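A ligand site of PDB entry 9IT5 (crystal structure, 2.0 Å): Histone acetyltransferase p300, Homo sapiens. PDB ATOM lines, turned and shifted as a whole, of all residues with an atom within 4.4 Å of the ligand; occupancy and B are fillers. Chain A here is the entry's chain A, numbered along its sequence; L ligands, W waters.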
ATOM      1  N   PHE A  89      21.322  18.969  -8.228  1.00  0.00           N
ATOM      2  CA  PHE A  89      19.899  19.253  -8.331  1.00  0.00           C
ATOM      3  C   PHE A  89      19.186  18.053  -8.945  1.00  0.00           C
ATOM      4  O   PHE A  89      19.656  17.482  -9.932  1.00  0.00           O
ATOM      5  CB  PHE A  89      19.624  20.508  -9.163  1.00  0.00           C
ATOM      6  CG  PHE A  89      18.151  20.808  -9.410  1.00  0.00           C
ATOM      7  CD1 PHE A  89      17.482  20.286 -10.516  1.00  0.00           C
ATOM      8  CD2 PHE A  89      17.429  21.604  -8.523  1.00  0.00           C
ATOM      9  CE1 PHE A  89      16.134  20.559 -10.731  1.00  0.00           C
ATOM     10  CE2 PHE A  89      16.081  21.876  -8.738  1.00  0.00           C
ATOM     11  CZ  PHE A  89      15.441  21.358  -9.850  1.00  0.00           C
ATOM     12  N   LEU A 113      11.718  17.806  -5.077  1.00  0.00           N
ATOM     13  CA  LEU A 113      12.941  18.515  -5.416  1.00  0.00           C
ATOM     14  C   LEU A 113      14.020  18.066  -4.448  1.00  0.00           C
ATOM     15  O   LEU A 113      13.723  17.838  -3.260  1.00  0.00           O
ATOM     16  CB  LEU A 113      12.756  20.030  -5.279  1.00  0.00           C
ATOM     17  CG  LEU A 113      11.755  20.715  -6.219  1.00  0.00           C
ATOM     18  CD1 LEU A 113      11.799  22.215  -5.943  1.00  0.00           C
ATOM     19  CD2 LEU A 113      12.064  20.399  -7.666  1.00  0.00           C
ATOM     20  N   ASP A 114      15.262  17.952  -4.919  1.00  0.00           N
ATOM     21  CA  ASP A 114      16.378  17.701  -4.025  1.00  0.00           C
ATOM     22  C   ASP A 114      17.582  18.462  -4.542  1.00  0.00           C
ATOM     23  O   ASP A 114      17.635  18.881  -5.688  1.00  0.00           O
ATOM     24  CB  ASP A 114      16.606  16.221  -3.778  1.00  0.00           C
ATOM     25  CG  ASP A 114      17.282  15.871  -2.446  1.00  0.00           C
ATOM     26  OD1 ASP A 114      17.805  16.788  -1.794  1.00  0.00           O
ATOM     27  OD2 ASP A 114      17.236  14.678  -2.053  1.00  0.00           O
ATOM     28  N   SER A 115      18.538  18.688  -3.642  1.00  0.00           N
ATOM     29  CA  SER A 115      19.742  19.417  -4.006  1.00  0.00           C
ATOM     30  C   SER A 115      20.890  19.036  -3.086  1.00  0.00           C
ATOM     31  O   SER A 115      20.656  18.521  -1.985  1.00  0.00           O
ATOM     32  CB  SER A 115      19.500  20.913  -4.020  1.00  0.00           C
ATOM     33  OG  SER A 115      19.221  21.434  -2.724  1.00  0.00           O
ATOM     34  N   TYR A 129      18.819  27.492  -9.363  1.00  0.00           N
ATOM     35  CA  TYR A 129      17.649  26.717  -8.986  1.00  0.00           C
ATOM     36  C   TYR A 129      16.400  27.326  -9.627  1.00  0.00           C
ATOM     37  O   TYR A 129      15.573  26.611 -10.203  1.00  0.00           O
ATOM     38  CB  TYR A 129      17.473  26.667  -7.468  1.00  0.00           C
ATOM     39  CG  TYR A 129      18.532  25.886  -6.708  1.00  0.00           C
ATOM     40  CD1 TYR A 129      19.238  24.823  -7.294  1.00  0.00           C
ATOM     41  CD2 TYR A 129      18.803  26.178  -5.387  1.00  0.00           C
ATOM     42  CE1 TYR A 129      20.195  24.111  -6.566  1.00  0.00           C
ATOM     43  CE2 TYR A 129      19.746  25.465  -4.660  1.00  0.00           C
ATOM     44  CZ  TYR A 129      20.445  24.426  -5.246  1.00  0.00           C
ATOM     45  OH  TYR A 129      21.371  23.764  -4.494  1.00  0.00           O
ATOM     46  N   CYS A 153       6.138  22.366   1.146  1.00  0.00           N
ATOM     47  CA  CYS A 153       6.580  22.057   2.488  1.00  0.00           C
ATOM     48  C   CYS A 153       8.054  21.687   2.483  1.00  0.00           C
ATOM     49  O   CYS A 153       8.571  21.216   1.462  1.00  0.00           O
ATOM     50  CB  CYS A 153       5.753  20.942   3.117  1.00  0.00           C
ATOM     51  SG  CYS A 153       6.030  19.334   2.352  1.00  0.00           S
ATOM     52  N   PRO A 154       8.759  21.854   3.634  1.00  0.00           N
ATOM     53  CA  PRO A 154      10.182  21.557   3.730  1.00  0.00           C
ATOM     54  C   PRO A 154      10.457  20.074   3.924  1.00  0.00           C
ATOM     55  O   PRO A 154       9.597  19.331   4.404  1.00  0.00           O
ATOM     56  CB  PRO A 154      10.695  22.365   4.935  1.00  0.00           C
ATOM     57  CG  PRO A 154       9.467  23.031   5.525  1.00  0.00           C
ATOM     58  CD  PRO A 154       8.228  22.399   4.896  1.00  0.00           C
ATOM     59  N   PRO A 155      11.689  19.628   3.619  1.00  0.00           N
ATOM     60  CA  PRO A 155      12.097  18.235   3.849  1.00  0.00           C
ATOM     61  C   PRO A 155      12.413  18.028   5.322  1.00  0.00           C
ATOM     62  O   PRO A 155      12.421  18.984   6.092  1.00  0.00           O
ATOM     63  CB  PRO A 155      13.335  18.128   2.963  1.00  0.00           C
ATOM     64  CG  PRO A 155      13.977  19.478   3.128  1.00  0.00           C
ATOM     65  CD  PRO A 155      12.794  20.444   3.109  1.00  0.00           C
ATOM     66  N   GLU A 157      15.189  15.963   7.990  1.00  0.00           N
ATOM     67  CA  GLU A 157      16.495  15.309   8.093  1.00  0.00           C
ATOM     68  C   GLU A 157      16.309  13.786   8.051  1.00  0.00           C
ATOM     69  O   GLU A 157      17.154  13.066   7.521  1.00  0.00           O
ATOM     70  CB  GLU A 157      17.219  15.748   9.364  1.00  0.00           C
ATOM     71  CG  GLU A 157      17.684  17.205   9.307  1.00  0.00           C
ATOM     72  CD  GLU A 157      18.205  17.737  10.630  1.00  0.00           C
ATOM     73  OE1 GLU A 157      19.153  17.113  11.155  1.00  0.00           O
ATOM     74  OE2 GLU A 157      17.678  18.760  11.123  1.00  0.00           O
ATOM     75  N   TYR A 161      14.928  12.774   0.161  1.00  0.00           N
ATOM     76  CA  TYR A 161      14.077  12.688  -1.018  1.00  0.00           C
ATOM     77  C   TYR A 161      14.757  11.909  -2.139  1.00  0.00           C
ATOM     78  O   TYR A 161      14.208  10.896  -2.594  1.00  0.00           O
ATOM     79  CB  TYR A 161      13.666  14.058  -1.589  1.00  0.00           C
ATOM     80  CG  TYR A 161      12.629  14.800  -0.761  1.00  0.00           C
ATOM     81  CD1 TYR A 161      11.900  14.166   0.242  1.00  0.00           C
ATOM     82  CD2 TYR A 161      12.379  16.142  -1.003  1.00  0.00           C
ATOM     83  CE1 TYR A 161      10.949  14.852   0.982  1.00  0.00           C
ATOM     84  CE2 TYR A 161      11.456  16.841  -0.253  1.00  0.00           C
ATOM     85  CZ  TYR A 161      10.733  16.200   0.746  1.00  0.00           C
ATOM     86  OH  TYR A 161       9.793  16.882   1.452  1.00  0.00           O
ATOM     87  N   HIS A 166      22.748  14.123   3.113  1.00  0.00           N
ATOM     88  CA  HIS A 166      22.964  15.506   2.734  1.00  0.00           C
ATOM     89  C   HIS A 166      24.084  16.100   3.581  1.00  0.00           C
ATOM     90  O   HIS A 166      24.431  15.553   4.620  1.00  0.00           O
ATOM     91  CB  HIS A 166      21.683  16.322   2.921  1.00  0.00           C
ATOM     92  CG  HIS A 166      20.634  16.079   1.878  1.00  0.00           C
ATOM     93  ND1 HIS A 166      19.782  15.001   1.925  1.00  0.00           N
ATOM     94  CD2 HIS A 166      20.317  16.771   0.760  1.00  0.00           C
ATOM     95  CE1 HIS A 166      18.964  15.043   0.872  1.00  0.00           C
ATOM     96  NE2 HIS A 166      19.290  16.100   0.130  1.00  0.00           N
ATOM     97  N   PRO A 167      24.670  17.252   3.185  1.00  0.00           N
ATOM     98  CA  PRO A 167      25.627  17.960   4.030  1.00  0.00           C
ATOM     99  C   PRO A 167      25.016  18.332   5.375  1.00  0.00           C
ATOM    100  O   PRO A 167      23.901  18.845   5.422  1.00  0.00           O
ATOM    101  CB  PRO A 167      26.025  19.192   3.217  1.00  0.00           C
ATOM    102  CG  PRO A 167      25.679  18.828   1.783  1.00  0.00           C
ATOM    103  CD  PRO A 167      24.462  17.923   1.885  1.00  0.00           C
ATOM    104  N   PRO A 168      25.718  18.106   6.514  1.00  0.00           N
ATOM    105  CA  PRO A 168      25.167  18.453   7.818  1.00  0.00           C
ATOM    106  C   PRO A 168      24.866  19.933   7.982  1.00  0.00           C
ATOM    107  O   PRO A 168      24.104  20.300   8.880  1.00  0.00           O
ATOM    108  CB  PRO A 168      26.221  17.945   8.821  1.00  0.00           C
ATOM    109  CG  PRO A 168      27.495  17.784   8.012  1.00  0.00           C
ATOM    110  CD  PRO A 168      27.041  17.482   6.589  1.00  0.00           C
ATOM    111  N   GLN A 170      23.767  21.838   5.213  1.00  0.00           N
ATOM    112  CA  GLN A 170      22.750  22.255   4.267  1.00  0.00           C
ATOM    113  C   GLN A 170      21.487  22.610   5.055  1.00  0.00           C
ATOM    114  O   GLN A 170      20.945  21.770   5.776  1.00  0.00           O
ATOM    115  CB  GLN A 170      22.516  21.201   3.176  1.00  0.00           C
ATOM    116  CG  GLN A 170      21.647  21.701   2.017  1.00  0.00           C
ATOM    117  CD  GLN A 170      21.660  20.794   0.799  1.00  0.00           C
ATOM    118  OE1 GLN A 170      22.706  20.319   0.348  1.00  0.00           O
ATOM    119  NE2 GLN A 170      20.479  20.540   0.259  1.00  0.00           N
ATOM    120  N   LYS A 171      21.022  23.845   4.894  1.00  0.00           N
ATOM    121  CA  LYS A 171      20.032  24.468   5.756  1.00  0.00           C
ATOM    122  C   LYS A 171      18.619  24.150   5.262  1.00  0.00           C
ATOM    123  O   LYS A 171      18.265  24.462   4.122  1.00  0.00           O
ATOM    124  CB  LYS A 171      20.239  25.986   5.717  1.00  0.00           C
ATOM    125  CG  LYS A 171      21.501  26.491   6.408  1.00  0.00           C
ATOM    126  CD  LYS A 171      21.423  26.410   7.931  1.00  0.00           C
ATOM    127  CE  LYS A 171      22.505  27.164   8.666  1.00  0.00           C
ATOM    128  NZ  LYS A 171      23.717  26.354   8.848  1.00  0.00           N
ATOM    129  N   ILE A 172      17.809  23.528   6.127  1.00  0.00           N
ATOM    130  CA  ILE A 172      16.410  23.280   5.806  1.00  0.00           C
ATOM    131  C   ILE A 172      15.611  24.544   6.104  1.00  0.00           C
ATOM    132  O   ILE A 172      15.619  25.041   7.223  1.00  0.00           O
ATOM    133  CB  ILE A 172      15.902  22.050   6.576  1.00  0.00           C
ATOM    134  CG1 ILE A 172      16.611  20.786   6.100  1.00  0.00           C
ATOM    135  CG2 ILE A 172      14.376  21.928   6.478  1.00  0.00           C
ATOM    136  CD1 ILE A 172      16.245  19.530   6.871  1.00  0.00           C
ATOM    137  N   PRO A 173      14.867  25.121   5.144  1.00  0.00           N
ATOM    138  CA  PRO A 173      14.105  26.337   5.431  1.00  0.00           C
ATOM    139  C   PRO A 173      12.937  26.004   6.356  1.00  0.00           C
ATOM    140  O   PRO A 173      12.451  24.873   6.365  1.00  0.00           O
ATOM    141  CB  PRO A 173      13.675  26.773   4.044  1.00  0.00           C
ATOM    142  CG  PRO A 173      13.477  25.471   3.313  1.00  0.00           C
ATOM    143  CD  PRO A 173      14.678  24.650   3.760  1.00  0.00           C
ATOM    144  N   LEU A 178      10.410  29.196   3.020  1.00  0.00           N
ATOM    145  CA  LEU A 178      10.272  28.376   1.822  1.00  0.00           C
ATOM    146  C   LEU A 178       9.190  28.956   0.910  1.00  0.00           C
ATOM    147  O   LEU A 178       9.360  29.023  -0.317  1.00  0.00           O
ATOM    148  CB  LEU A 178       9.935  26.936   2.194  1.00  0.00           C
ATOM    149  CG  LEU A 178       9.777  25.943   1.052  1.00  0.00           C
ATOM    150  CD1 LEU A 178      11.018  25.897   0.220  1.00  0.00           C
ATOM    151  CD2 LEU A 178       9.451  24.564   1.615  1.00  0.00           C
ATOM    152  N   TRP A 181      10.558  31.834  -0.888  1.00  0.00           N
ATOM    153  CA  TRP A 181      11.439  31.351  -1.936  1.00  0.00           C
ATOM    154  C   TRP A 181      10.645  31.036  -3.206  1.00  0.00           C
ATOM    155  O   TRP A 181      11.042  31.395  -4.317  1.00  0.00           O
ATOM    156  CB  TRP A 181      12.177  30.112  -1.423  1.00  0.00           C
ATOM    157  CG  TRP A 181      13.330  29.618  -2.259  1.00  0.00           C
ATOM    158  CD1 TRP A 181      14.656  29.897  -2.065  1.00  0.00           C
ATOM    159  CD2 TRP A 181      13.268  28.687  -3.361  1.00  0.00           C
ATOM    160  NE1 TRP A 181      15.412  29.240  -3.002  1.00  0.00           N
ATOM    161  CE2 TRP A 181      14.592  28.482  -3.803  1.00  0.00           C
ATOM    162  CE3 TRP A 181      12.237  28.007  -4.018  1.00  0.00           C
ATOM    163  CZ2 TRP A 181      14.904  27.636  -4.870  1.00  0.00           C
ATOM    164  CZ3 TRP A 181      12.546  27.164  -5.061  1.00  0.00           C
ATOM    165  CH2 TRP A 181      13.862  26.986  -5.479  1.00  0.00           C
ATOM    166  N   TYR A 182       9.525  30.317  -3.056  1.00  0.00           N
ATOM    167  CA  TYR A 182       8.741  29.906  -4.216  1.00  0.00           C
ATOM    168  C   TYR A 182       8.122  31.147  -4.863  1.00  0.00           C
ATOM    169  O   TYR A 182       8.043  31.234  -6.070  1.00  0.00           O
ATOM    170  CB  TYR A 182       7.686  28.855  -3.881  1.00  0.00           C
ATOM    171  CG  TYR A 182       8.173  27.418  -3.745  1.00  0.00           C
ATOM    172  CD1 TYR A 182       8.637  26.710  -4.837  1.00  0.00           C
ATOM    173  CD2 TYR A 182       8.124  26.748  -2.514  1.00  0.00           C
ATOM    174  CE1 TYR A 182       9.085  25.399  -4.730  1.00  0.00           C
ATOM    175  CE2 TYR A 182       8.557  25.427  -2.390  1.00  0.00           C
ATOM    176  CZ  TYR A 182       9.023  24.746  -3.503  1.00  0.00           C
ATOM    177  OH  TYR A 182       9.458  23.456  -3.408  1.00  0.00           O
HETATM  178  C1  LIG L   1      15.947  23.882  -5.263  1.00  0.00           C
HETATM  179  C2  LIG L   1      16.330  23.475  -3.842  1.00  0.00           C
HETATM  180  C3  LIG L   1      15.795  22.091  -3.471  1.00  0.00           C
HETATM  181  N1  LIG L   1      16.354  21.613  -2.195  1.00  0.00           N
HETATM  182  C4  LIG L   1      15.515  20.584  -1.578  1.00  0.00           C
HETATM  183  C5  LIG L   1      16.334  19.752  -0.597  1.00  0.00           C
HETATM  184  C6  LIG L   1      15.561  18.523  -0.112  1.00  0.00           C
HETATM  185  N2  LIG L   1      16.288  17.862   0.961  1.00  0.00           N
HETATM  186  C7  LIG L   1      17.104  18.571   1.793  1.00  0.00           C
HETATM  187  C8  LIG L   1      17.700  17.982   2.902  1.00  0.00           C
HETATM  188  C9  LIG L   1      18.496  18.749   3.729  1.00  0.00           C
HETATM  189  C10 LIG L   1      18.693  20.083   3.412  1.00  0.00           C
HETATM  190  N3  LIG L   1      18.100  20.672   2.349  1.00  0.00           N
HETATM  191  C11 LIG L   1      17.330  19.943   1.545  1.00  0.00           C
HETATM  192  O1  LIG L   1      16.759  20.602   0.486  1.00  0.00           O
HETATM  193  C12 LIG L   1      19.164  18.126   4.895  1.00  0.00           C
HETATM  194  C13 LIG L   1      19.021  16.802   5.335  1.00  0.00           C
HETATM  195  N4  LIG L   1      19.780  16.534   6.389  1.00  0.00           N
HETATM  196  N5  LIG L   1      20.418  17.711   6.656  1.00  0.00           N
HETATM  197  C14 LIG L   1      20.075  18.687   5.773  1.00  0.00           C
HETATM  198  C15 LIG L   1      21.337  17.783   7.789  1.00  0.00           C
HETATM  199  C16 LIG L   1      14.252  21.198  -0.997  1.00  0.00           C
HETATM  200  C17 LIG L   1      13.007  20.672  -1.323  1.00  0.00           C
HETATM  201  C18 LIG L   1      11.849  21.215  -0.813  1.00  0.00           C
HETATM  202  C19 LIG L   1      11.904  22.321  -0.006  1.00  0.00           C
HETATM  203  C20 LIG L   1      13.134  22.855   0.335  1.00  0.00           C
HETATM  204  C21 LIG L   1      14.296  22.292  -0.151  1.00  0.00           C
HETATM  205  C22 LIG L   1      15.889  24.504  -2.817  1.00  0.00           C
HETATM  206  C23 LIG L   1      14.556  24.894  -2.732  1.00  0.00           C
HETATM  207  C24 LIG L   1      14.137  25.816  -1.806  1.00  0.00           C
HETATM  208  C25 LIG L   1      15.047  26.356  -0.917  1.00  0.00           C
HETATM  209  C26 LIG L   1      16.384  25.994  -0.976  1.00  0.00           C
HETATM  210  C27 LIG L   1      16.790  25.063  -1.919  1.00  0.00           C
HETATM  211  C28 LIG L   1      14.604  27.331   0.045  1.00  0.00           C
HETATM  212  N6  LIG L   1      14.180  28.092   0.774  1.00  0.00           N
HETATM  213  O   HOH W   1      15.397  15.234   1.679  1.00  0.00           O
HETATM  214  O   HOH W   2      16.567  14.794   3.962  1.00  0.00           O
HETATM  215  O   HOH W   3      18.216  23.476   1.263  1.00  0.00           O
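Residues that only touch the ligand: Leu 113 (3.5 Å), Tyr 129 (3.6 Å), Cys 153 (3.8 Å), Pro 155 (3.5 Å), Glu 157 (3.7 Å), His 166 (3.6 Å), Pro 167 (3.6 Å), Pro 168 (3.9 Å), Ile 172 (3.5 Å), Pro 173 (3.6 Å), Leu 178 (3.7 Å) and Trp 181 (3.3 Å). 15 residues have an atom within 4 Å of the ligand: Leu 113, Asp 114, Ser 115, Tyr 129, Cys 153, Pro 155, Glu 157, His 166, Pro 167, Pro 168, Gln 170, Ile 172, Pro 173, Leu 178 and Trp 181.
The side-chain amide nitrogen (NE2) of Gln 170 lies within hydrogen-bond range of the backbone carbonyl oxygen (O) of Ser 115 (3.0 Å). O of Ser 115 lies close to NE2 of His 166 (3.5 Å). A ring nitrogen (NE2) of His 166 is in hydrogen-bond range of the side-chain carboxylate (OD1) of Asp 114 (2.5 Å).
Water W1 lies within hydrogen-bond range of N2 of the ligand (2.9 Å) and N of Tyr 161 (2.9 Å). Water W3 lies within hydrogen-bond range of N3 of the ligand and O of Lys 171.
The side-chain hydroxyl (OG) of Ser 115 sits at hydrogen-bond distance from a nitrogen (N1) of the ligand. NE2 of Gln 170 is in hydrogen-bond range of N3 of the ligand (3.2 Å). A nitrogen (N2) of the ligand sits close to the side-chain carboxylate (OD1) of Asp 114, at 3.3 Å.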
